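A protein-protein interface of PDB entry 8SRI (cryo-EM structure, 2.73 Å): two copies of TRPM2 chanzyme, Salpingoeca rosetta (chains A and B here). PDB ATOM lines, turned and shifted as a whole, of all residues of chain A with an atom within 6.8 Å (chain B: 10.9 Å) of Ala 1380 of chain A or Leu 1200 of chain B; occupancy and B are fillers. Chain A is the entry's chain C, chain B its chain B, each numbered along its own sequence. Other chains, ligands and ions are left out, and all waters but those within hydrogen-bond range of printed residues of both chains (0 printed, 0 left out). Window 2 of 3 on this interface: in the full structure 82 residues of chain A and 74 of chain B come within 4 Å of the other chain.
No position is printed for both chains.
Of chain B, only Leu 1200 (3.9 Å), Asn 1201 (3.6 Å) and Ser 1202 (2.7 Å) come within 4 Å of Ala 1380 of chain A. Leu 1200 of chain B touches just these residues of chain A: Ala 1380, Gly 1416, Ile 1418 and Val 1440. No residue of chain B comes within 4 Å of Asp 1378 of chain A. No residue of chain B comes within 4 Å of Val 1379 of chain A. Leu 1381 of chain A touches one residue of chain B. No residue of chain B comes within 4 Å of Thr 1382 of chain A. Of the printed residues of chain B, Ser 1383 of chain A touches Ser 1202. No residue of chain B comes within 4 Å of Ser 1414 of chain A. Gly 1416 of chain A touches just these residues of chain B: Asn 1198 (3.6 Å), Arg 1199 (3.8 Å) and Leu 1200 (3.0 Å). Printed residues of chain A within 4 Å of Asn 1201 of chain B: Ala 1380 (3.6 Å). Printed residues of chain B within 4 Å of Arg 1385 of chain A: Ala 1205 (3.7 Å). The nearest residue of chain B that does not touch Ala 1380 of chain A is Ala 1205 of chain B (4.5 Å).
O of Val 1379 of chain A sits at hydrogen-bond distance from OG of Ser 1383 of chain A. OD1 of Asn 1201 of chain B sits at hydrogen-bond distance from N of Ala 1203 of chain B (3.3 Å). OG of Ser 1383 of chain A sits at hydrogen-bond distance from O of Ala 1380 of chain A, 2.6 Å away. The side-chain hydroxyl of Thr 1331 of chain A lies within hydrogen-bond range of the backbone carbonyl oxygen of Ser 1383 of chain A (2.7 Å).
The backbone carbonyl oxygen (O) of Ala 1380 of chain A lies within hydrogen-bond range of the side-chain hydroxyl (OG) of Ser 1202 of chain B (2.7 Å). O of Phe 1413 of chain A is in hydrogen-bond range of N of Ser 1202 of chain B, at 3.4 Å. N of Leu 1200 of chain B is in hydrogen-bond range of O of Gly 1416 of chain A, 3.0 Å away. The backbone carbonyl oxygen (O) of Asn 1198 of chain B lies within hydrogen-bond range of the backbone NH (N) of Ile 1418 of chain A, at 3.2 Å.
Along chain A the printed residues that touch a printed residue of chain B span positions 1380 to 1442. Among the printed residues, 18 pairs touch across the chains. Among the printed residues, no Asp or Glu carboxylate lies within 4 Å of a Lys or Arg side-chain nitrogen of the other chain.
CD1 of Leu 1200 of chain B touches CB of Ala 1380 of chain A, at 3.9 Å. CB of Ala 1380 of chain A touches O of Asn 1201 of chain B, at 3.6 Å. O of Leu 1381 of chain A touches CB of Ala 1205 of chain B, 3.6 Å away. Ser 1202 of chain B touches Gly 1384 of chain A (OG to CA, 3.7 Å). Gly 1384 of chain A touches Ala 1205 of chain B. Ala 1205 of chain B touches Arg 1385 of chain A. Arg 1199 of chain B touches Gly 1416 of chain A. Asn 1198 of chain B touches Thr 1417 of chain A (O to CA, 3.4 Å). Val 1440 of chain A touches Leu 1200 of chain B (CG1 to CD2, 3.9 Å). Phe 1442 of chain A touches Ser 1202 of chain B (CZ to CB, 3.7 Å).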
ATOM      1  N   ALA A1329     -12.702  26.427  -2.024  1.00  0.00           N
ATOM      2  CA  ALA A1329     -12.065  26.535  -0.724  1.00  0.00           C
ATOM      3  C   ALA A1329     -12.641  27.740  -0.008  1.00  0.00           C
ATOM      4  O   ALA A1329     -12.701  28.837  -0.575  1.00  0.00           O
ATOM      5  CB  ALA A1329     -10.551  26.686  -0.861  1.00  0.00           C
ATOM      6  N   THR A1331     -12.490  30.076   3.620  1.00  0.00           N
ATOM      7  CA  THR A1331     -11.585  30.504   4.680  1.00  0.00           C
ATOM      8  C   THR A1331     -12.412  31.103   5.809  1.00  0.00           C
ATOM      9  O   THR A1331     -12.962  32.199   5.662  1.00  0.00           O
ATOM     10  CB  THR A1331     -10.605  31.536   4.123  1.00  0.00           C
ATOM     11  OG1 THR A1331     -10.077  31.080   2.870  1.00  0.00           O
ATOM     12  CG2 THR A1331      -9.491  31.827   5.090  1.00  0.00           C
ATOM     13  N   GLU A1377      -2.647  24.693  -8.699  1.00  0.00           N
ATOM     14  CA  GLU A1377      -2.539  25.113  -7.309  1.00  0.00           C
ATOM     15  C   GLU A1377      -3.423  24.264  -6.403  1.00  0.00           C
ATOM     16  O   GLU A1377      -4.363  23.604  -6.852  1.00  0.00           O
ATOM     17  CB  GLU A1377      -2.915  26.590  -7.155  1.00  0.00           C
ATOM     18  N   ASP A1378      -3.104  24.294  -5.107  1.00  0.00           N
ATOM     19  CA  ASP A1378      -3.767  23.478  -4.102  1.00  0.00           C
ATOM     20  C   ASP A1378      -4.746  24.345  -3.298  1.00  0.00           C
ATOM     21  O   ASP A1378      -4.894  25.543  -3.554  1.00  0.00           O
ATOM     22  CB  ASP A1378      -2.725  22.760  -3.240  1.00  0.00           C
ATOM     23  CG  ASP A1378      -1.759  23.709  -2.578  1.00  0.00           C
ATOM     24  OD1 ASP A1378      -0.943  24.326  -3.293  1.00  0.00           O
ATOM     25  OD2 ASP A1378      -1.786  23.807  -1.340  1.00  0.00           O
ATOM     26  N   VAL A1379      -5.440  23.715  -2.340  1.00  0.00           N
ATOM     27  CA  VAL A1379      -6.473  24.374  -1.527  1.00  0.00           C
ATOM     28  C   VAL A1379      -5.940  25.436  -0.540  1.00  0.00           C
ATOM     29  O   VAL A1379      -6.634  26.447  -0.298  1.00  0.00           O
ATOM     30  CB  VAL A1379      -7.232  23.212  -0.825  1.00  0.00           C
ATOM     31  CG1 VAL A1379      -8.434  23.635   0.019  1.00  0.00           C
ATOM     32  CG2 VAL A1379      -7.672  22.154  -1.847  1.00  0.00           C
ATOM     33  N   ALA A1380      -4.717  25.234   0.003  1.00  0.00           N
ATOM     34  CA  ALA A1380      -4.039  26.128   0.970  1.00  0.00           C
ATOM     35  C   ALA A1380      -3.790  27.545   0.437  1.00  0.00           C
ATOM     36  O   ALA A1380      -4.215  28.544   1.056  1.00  0.00           O
ATOM     37  CB  ALA A1380      -2.726  25.502   1.437  1.00  0.00           C
ATOM     38  N   LEU A1381      -3.160  27.613  -0.756  1.00  0.00           N
ATOM     39  CA  LEU A1381      -2.844  28.853  -1.468  1.00  0.00           C
ATOM     40  C   LEU A1381      -4.116  29.548  -1.925  1.00  0.00           C
ATOM     41  O   LEU A1381      -4.161  30.785  -1.916  1.00  0.00           O
ATOM     42  CB  LEU A1381      -1.899  28.558  -2.643  1.00  0.00           C
ATOM     43  CG  LEU A1381      -1.439  29.645  -3.630  1.00  0.00           C
ATOM     44  CD1 LEU A1381       0.058  29.507  -3.869  1.00  0.00           C
ATOM     45  CD2 LEU A1381      -2.170  29.614  -4.971  1.00  0.00           C
ATOM     46  N   THR A1382      -5.102  28.754  -2.410  1.00  0.00           N
ATOM     47  CA  THR A1382      -6.351  29.256  -2.991  1.00  0.00           C
ATOM     48  C   THR A1382      -7.182  29.952  -1.917  1.00  0.00           C
ATOM     49  O   THR A1382      -7.671  31.069  -2.144  1.00  0.00           O
ATOM     50  CB  THR A1382      -7.144  28.107  -3.612  1.00  0.00           C
ATOM     51  OG1 THR A1382      -6.302  27.359  -4.500  1.00  0.00           O
ATOM     52  CG2 THR A1382      -8.359  28.620  -4.360  1.00  0.00           C
ATOM     53  N   SER A1383      -7.277  29.291  -0.737  1.00  0.00           N
ATOM     54  CA  SER A1383      -8.013  29.742   0.452  1.00  0.00           C
ATOM     55  C   SER A1383      -7.429  31.051   0.976  1.00  0.00           C
ATOM     56  O   SER A1383      -8.170  32.020   1.239  1.00  0.00           O
ATOM     57  CB  SER A1383      -7.983  28.660   1.532  1.00  0.00           C
ATOM     58  OG  SER A1383      -6.670  28.479   2.034  1.00  0.00           O
ATOM     59  N   GLY A1384      -6.085  31.053   1.137  1.00  0.00           N
ATOM     60  CA  GLY A1384      -5.345  32.229   1.588  1.00  0.00           C
ATOM     61  C   GLY A1384      -5.427  33.403   0.620  1.00  0.00           C
ATOM     62  O   GLY A1384      -5.614  34.544   1.056  1.00  0.00           O
ATOM     63  N   ARG A1385      -5.266  33.118  -0.698  1.00  0.00           N
ATOM     64  CA  ARG A1385      -5.287  34.101  -1.793  1.00  0.00           C
ATOM     65  C   ARG A1385      -6.651  34.786  -1.896  1.00  0.00           C
ATOM     66  O   ARG A1385      -6.715  36.008  -2.107  1.00  0.00           O
ATOM     67  CB  ARG A1385      -4.896  33.417  -3.109  1.00  0.00           C
ATOM     68  CG  ARG A1385      -4.809  34.339  -4.327  1.00  0.00           C
ATOM     69  CD  ARG A1385      -4.481  33.584  -5.620  1.00  0.00           C
ATOM     70  NE  ARG A1385      -5.243  32.352  -5.807  1.00  0.00           N
ATOM     71  CZ  ARG A1385      -6.471  32.280  -6.307  1.00  0.00           C
ATOM     72  NH1 ARG A1385      -7.135  33.363  -6.682  1.00  0.00           N
ATOM     73  NH2 ARG A1385      -7.046  31.090  -6.445  1.00  0.00           N
ATOM     74  N   PHE A1413      -1.879  32.361   9.578  1.00  0.00           N
ATOM     75  CA  PHE A1413      -2.084  31.356   8.554  1.00  0.00           C
ATOM     76  C   PHE A1413      -1.270  30.097   8.852  1.00  0.00           C
ATOM     77  O   PHE A1413      -1.396  29.113   8.117  1.00  0.00           O
ATOM     78  CB  PHE A1413      -1.708  31.899   7.160  1.00  0.00           C
ATOM     79  CG  PHE A1413      -2.792  32.720   6.457  1.00  0.00           C
ATOM     80  CD1 PHE A1413      -3.941  33.208   7.124  1.00  0.00           C
ATOM     81  CD2 PHE A1413      -2.619  33.025   5.097  1.00  0.00           C
ATOM     82  CE1 PHE A1413      -4.905  33.967   6.440  1.00  0.00           C
ATOM     83  CE2 PHE A1413      -3.567  33.792   4.400  1.00  0.00           C
ATOM     84  CZ  PHE A1413      -4.712  34.255   5.075  1.00  0.00           C
ATOM     85  N   SER A1414      -0.437  30.097   9.917  1.00  0.00           N
ATOM     86  CA  SER A1414       0.376  28.919  10.192  1.00  0.00           C
ATOM     87  C   SER A1414      -0.367  27.817  10.939  1.00  0.00           C
ATOM     88  O   SER A1414       0.137  26.690  10.989  1.00  0.00           O
ATOM     89  CB  SER A1414       1.620  29.321  10.987  1.00  0.00           C
ATOM     90  N   SER A1415      -1.533  28.094  11.524  1.00  0.00           N
ATOM     91  CA  SER A1415      -2.281  27.085  12.279  1.00  0.00           C
ATOM     92  C   SER A1415      -3.709  26.973  11.745  1.00  0.00           C
ATOM     93  O   SER A1415      -4.612  27.650  12.243  1.00  0.00           O
ATOM     94  CB  SER A1415      -2.269  27.418  13.769  1.00  0.00           C
ATOM     95  N   GLY A1416      -3.917  26.136  10.738  1.00  0.00           N
ATOM     96  CA  GLY A1416      -5.243  25.913  10.177  1.00  0.00           C
ATOM     97  C   GLY A1416      -5.635  24.449  10.178  1.00  0.00           C
ATOM     98  O   GLY A1416      -4.801  23.576   9.929  1.00  0.00           O
ATOM     99  N   THR A1417      -6.912  24.186  10.461  1.00  0.00           N
ATOM    100  CA  THR A1417      -7.456  22.832  10.507  1.00  0.00           C
ATOM    101  C   THR A1417      -8.570  22.705   9.476  1.00  0.00           C
ATOM    102  O   THR A1417      -9.480  23.540   9.444  1.00  0.00           O
ATOM    103  CB  THR A1417      -8.005  22.486  11.901  1.00  0.00           C
ATOM    104  OG1 THR A1417      -9.069  23.385  12.239  1.00  0.00           O
ATOM    105  CG2 THR A1417      -6.917  22.546  12.979  1.00  0.00           C
ATOM    106  N   ILE A1418      -8.488  21.684   8.623  1.00  0.00           N
ATOM    107  CA  ILE A1418      -9.546  21.403   7.654  1.00  0.00           C
ATOM    108  C   ILE A1418     -10.690  20.745   8.426  1.00  0.00           C
ATOM    109  O   ILE A1418     -10.546  19.629   8.936  1.00  0.00           O
ATOM    110  CB  ILE A1418      -9.050  20.518   6.502  1.00  0.00           C
ATOM    111  CG1 ILE A1418      -8.036  21.295   5.652  1.00  0.00           C
ATOM    112  CG2 ILE A1418     -10.228  20.097   5.602  1.00  0.00           C
ATOM    113  CD1 ILE A1418      -7.439  20.513   4.478  1.00  0.00           C
ATOM    114  N   THR A1438     -14.195  22.632   0.489  1.00  0.00           N
ATOM    115  CA  THR A1438     -13.282  22.302   1.570  1.00  0.00           C
ATOM    116  C   THR A1438     -13.188  23.540   2.455  1.00  0.00           C
ATOM    117  O   THR A1438     -12.898  24.641   1.965  1.00  0.00           O
ATOM    118  CB  THR A1438     -11.908  21.903   1.019  1.00  0.00           C
ATOM    119  OG1 THR A1438     -12.034  20.698   0.255  1.00  0.00           O
ATOM    120  CG2 THR A1438     -10.913  21.641   2.142  1.00  0.00           C
ATOM    121  N   CYS A1439     -13.454  23.367   3.747  1.00  0.00           N
ATOM    122  CA  CYS A1439     -13.480  24.471   4.693  1.00  0.00           C
ATOM    123  C   CYS A1439     -12.220  24.463   5.548  1.00  0.00           C
ATOM    124  O   CYS A1439     -11.892  23.441   6.160  1.00  0.00           O
ATOM    125  CB  CYS A1439     -14.720  24.361   5.577  1.00  0.00           C
ATOM    126  SG  CYS A1439     -14.993  25.743   6.672  1.00  0.00           S
ATOM    127  N   VAL A1440     -11.514  25.596   5.590  1.00  0.00           N
ATOM    128  CA  VAL A1440     -10.296  25.730   6.383  1.00  0.00           C
ATOM    129  C   VAL A1440     -10.562  26.781   7.451  1.00  0.00           C
ATOM    130  O   VAL A1440     -10.936  27.920   7.134  1.00  0.00           O
ATOM    131  CB  VAL A1440      -9.070  26.131   5.539  1.00  0.00           C
ATOM    132  CG1 VAL A1440      -7.798  25.939   6.348  1.00  0.00           C
ATOM    133  CG2 VAL A1440      -8.981  25.351   4.226  1.00  0.00           C
ATOM    134  N   PHE A1442      -9.169  29.092  10.511  1.00  0.00           N
ATOM    135  CA  PHE A1442      -8.029  29.760  11.142  1.00  0.00           C
ATOM    136  C   PHE A1442      -8.502  30.425  12.428  1.00  0.00           C
ATOM    137  O   PHE A1442      -9.142  31.480  12.388  1.00  0.00           O
ATOM    138  CB  PHE A1442      -7.391  30.770  10.196  1.00  0.00           C
ATOM    139  CG  PHE A1442      -6.787  30.154   8.976  1.00  0.00           C
ATOM    140  CD1 PHE A1442      -5.592  29.420   9.076  1.00  0.00           C
ATOM    141  CD2 PHE A1442      -7.428  30.270   7.736  1.00  0.00           C
ATOM    142  CE1 PHE A1442      -5.019  28.832   7.935  1.00  0.00           C
ATOM    143  CE2 PHE A1442      -6.873  29.682   6.586  1.00  0.00           C
ATOM    144  CZ  PHE A1442      -5.672  28.964   6.696  1.00  0.00           C
ATOM    145  N   ASN B1198      -5.921  17.095  10.575  1.00  0.00           N
ATOM    146  CA  ASN B1198      -5.935  17.770   9.282  1.00  0.00           C
ATOM    147  C   ASN B1198      -5.194  19.103   9.358  1.00  0.00           C
ATOM    148  O   ASN B1198      -5.780  20.168   9.164  1.00  0.00           O
ATOM    149  CB  ASN B1198      -7.372  17.980   8.810  1.00  0.00           C
ATOM    150  N   ARG B1199      -3.896  19.022   9.631  1.00  0.00           N
ATOM    151  CA  ARG B1199      -3.051  20.205   9.744  1.00  0.00           C
ATOM    152  C   ARG B1199      -2.650  20.731   8.370  1.00  0.00           C
ATOM    153  O   ARG B1199      -2.110  19.990   7.542  1.00  0.00           O
ATOM    154  CB  ARG B1199      -1.806  19.884  10.569  1.00  0.00           C
ATOM    155  N   LEU B1200      -2.914  22.015   8.127  1.00  0.00           N
ATOM    156  CA  LEU B1200      -2.705  22.636   6.825  1.00  0.00           C
ATOM    157  C   LEU B1200      -1.950  23.941   7.046  1.00  0.00           C
ATOM    158  O   LEU B1200      -2.256  24.694   7.975  1.00  0.00           O
ATOM    159  CB  LEU B1200      -4.044  22.889   6.108  1.00  0.00           C
ATOM    160  CG  LEU B1200      -4.025  23.442   4.679  1.00  0.00           C
ATOM    161  CD1 LEU B1200      -3.350  22.459   3.734  1.00  0.00           C
ATOM    162  CD2 LEU B1200      -5.429  23.774   4.201  1.00  0.00           C
ATOM    163  N   ASN B1201      -0.964  24.204   6.184  1.00  0.00           N
ATOM    164  CA  ASN B1201      -0.136  25.406   6.254  1.00  0.00           C
ATOM    165  C   ASN B1201      -0.430  26.241   5.006  1.00  0.00           C
ATOM    166  O   ASN B1201      -0.099  25.835   3.887  1.00  0.00           O
ATOM    167  CB  ASN B1201       1.338  25.000   6.365  1.00  0.00           C
ATOM    168  CG  ASN B1201       2.256  26.112   6.897  1.00  0.00           C
ATOM    169  OD1 ASN B1201       2.111  27.292   6.594  1.00  0.00           O
ATOM    170  ND2 ASN B1201       3.215  25.708   7.720  1.00  0.00           N
ATOM    171  N   SER B1202      -1.052  27.405   5.209  1.00  0.00           N
ATOM    172  CA  SER B1202      -1.455  28.318   4.142  1.00  0.00           C
ATOM    173  C   SER B1202      -0.598  29.583   4.065  1.00  0.00           C
ATOM    174  O   SER B1202      -1.044  30.586   3.498  1.00  0.00           O
ATOM    175  CB  SER B1202      -2.927  28.694   4.291  1.00  0.00           C
ATOM    176  OG  SER B1202      -3.315  29.640   3.310  1.00  0.00           O
ATOM    177  N   ALA B1203       0.608  29.569   4.653  1.00  0.00           N
ATOM    178  CA  ALA B1203       1.534  30.710   4.626  1.00  0.00           C
ATOM    179  C   ALA B1203       2.116  31.023   3.245  1.00  0.00           C
ATOM    180  O   ALA B1203       2.637  32.130   3.062  1.00  0.00           O
ATOM    181  CB  ALA B1203       2.683  30.489   5.611  1.00  0.00           C
ATOM    182  N   VAL B1204       2.114  30.052   2.312  1.00  0.00           N
ATOM    183  CA  VAL B1204       2.601  30.191   0.928  1.00  0.00           C
ATOM    184  C   VAL B1204       1.813  31.246   0.124  1.00  0.00           C
ATOM    185  O   VAL B1204       2.376  31.919  -0.752  1.00  0.00           O
ATOM    186  CB  VAL B1204       2.566  28.787   0.260  1.00  0.00           C
ATOM    187  CG1 VAL B1204       3.362  28.717  -1.055  1.00  0.00           C
ATOM    188  CG2 VAL B1204       3.067  27.702   1.222  1.00  0.00           C
ATOM    189  N   ALA B1205       0.521  31.450   0.447  1.00  0.00           N
ATOM    190  CA  ALA B1205      -0.350  32.465  -0.158  1.00  0.00           C
ATOM    191  C   ALA B1205       0.063  33.910   0.147  1.00  0.00           C
ATOM    192  O   ALA B1205      -0.281  34.814  -0.622  1.00  0.00           O
ATOM    193  CB  ALA B1205      -1.790  32.241   0.289  1.00  0.00           C
ATOM    194  N   VAL B1206       0.784  34.140   1.242  1.00  0.00           N
ATOM    195  CA  VAL B1206       1.157  35.478   1.701  1.00  0.00           C
ATOM    196  C   VAL B1206       2.519  35.864   1.128  1.00  0.00           C
ATOM    197  O   VAL B1206       2.674  36.921   0.509  1.00  0.00           O
ATOM    198  CB  VAL B1206       1.117  35.543   3.253  1.00  0.00           C
ATOM    199  CG1 VAL B1206       1.925  36.730   3.839  1.00  0.00           C
ATOM    200  CG2 VAL B1206      -0.314  35.583   3.749  1.00  0.00           C
ATOM    201  N   HIS B1207       3.519  35.001   1.324  1.00  0.00           N
ATOM    202  CA  HIS B1207       4.897  35.269   0.929  1.00  0.00           C
ATOM    203  C   HIS B1207       5.088  34.999  -0.560  1.00  0.00           C
ATOM    204  O   HIS B1207       5.492  35.887  -1.319  1.00  0.00           O
ATOM    205  CB  HIS B1207       5.856  34.412   1.761  1.00  0.00           C
ATOM    206  CG  HIS B1207       6.041  34.897   3.165  1.00  0.00           C
ATOM    207  ND1 HIS B1207       6.246  34.043   4.227  1.00  0.00           N
ATOM    208  CD2 HIS B1207       6.047  36.149   3.682  1.00  0.00           C
ATOM    209  CE1 HIS B1207       6.373  34.747   5.337  1.00  0.00           C
ATOM    210  NE2 HIS B1207       6.256  36.027   5.034  1.00  0.00           N
ATOM    211  N   GLY B1208       4.800  33.776  -0.992  1.00  0.00           N
ATOM    212  CA  GLY B1208       4.963  33.366  -2.371  1.00  0.00           C
ATOM    213  C   GLY B1208       6.053  32.347  -2.581  1.00  0.00           C
ATOM    214  O   GLY B1208       6.453  32.116  -3.729  1.00  0.00           O
ATOM    215  N   HIS B1209       6.524  31.725  -1.506  1.00  0.00           N
ATOM    216  CA  HIS B1209       7.454  30.607  -1.533  1.00  0.00           C
ATOM    217  C   HIS B1209       7.226  29.823  -0.250  1.00  0.00           C
ATOM    218  O   HIS B1209       6.322  30.126   0.532  1.00  0.00           O
ATOM    219  CB  HIS B1209       8.909  31.072  -1.649  1.00  0.00           C
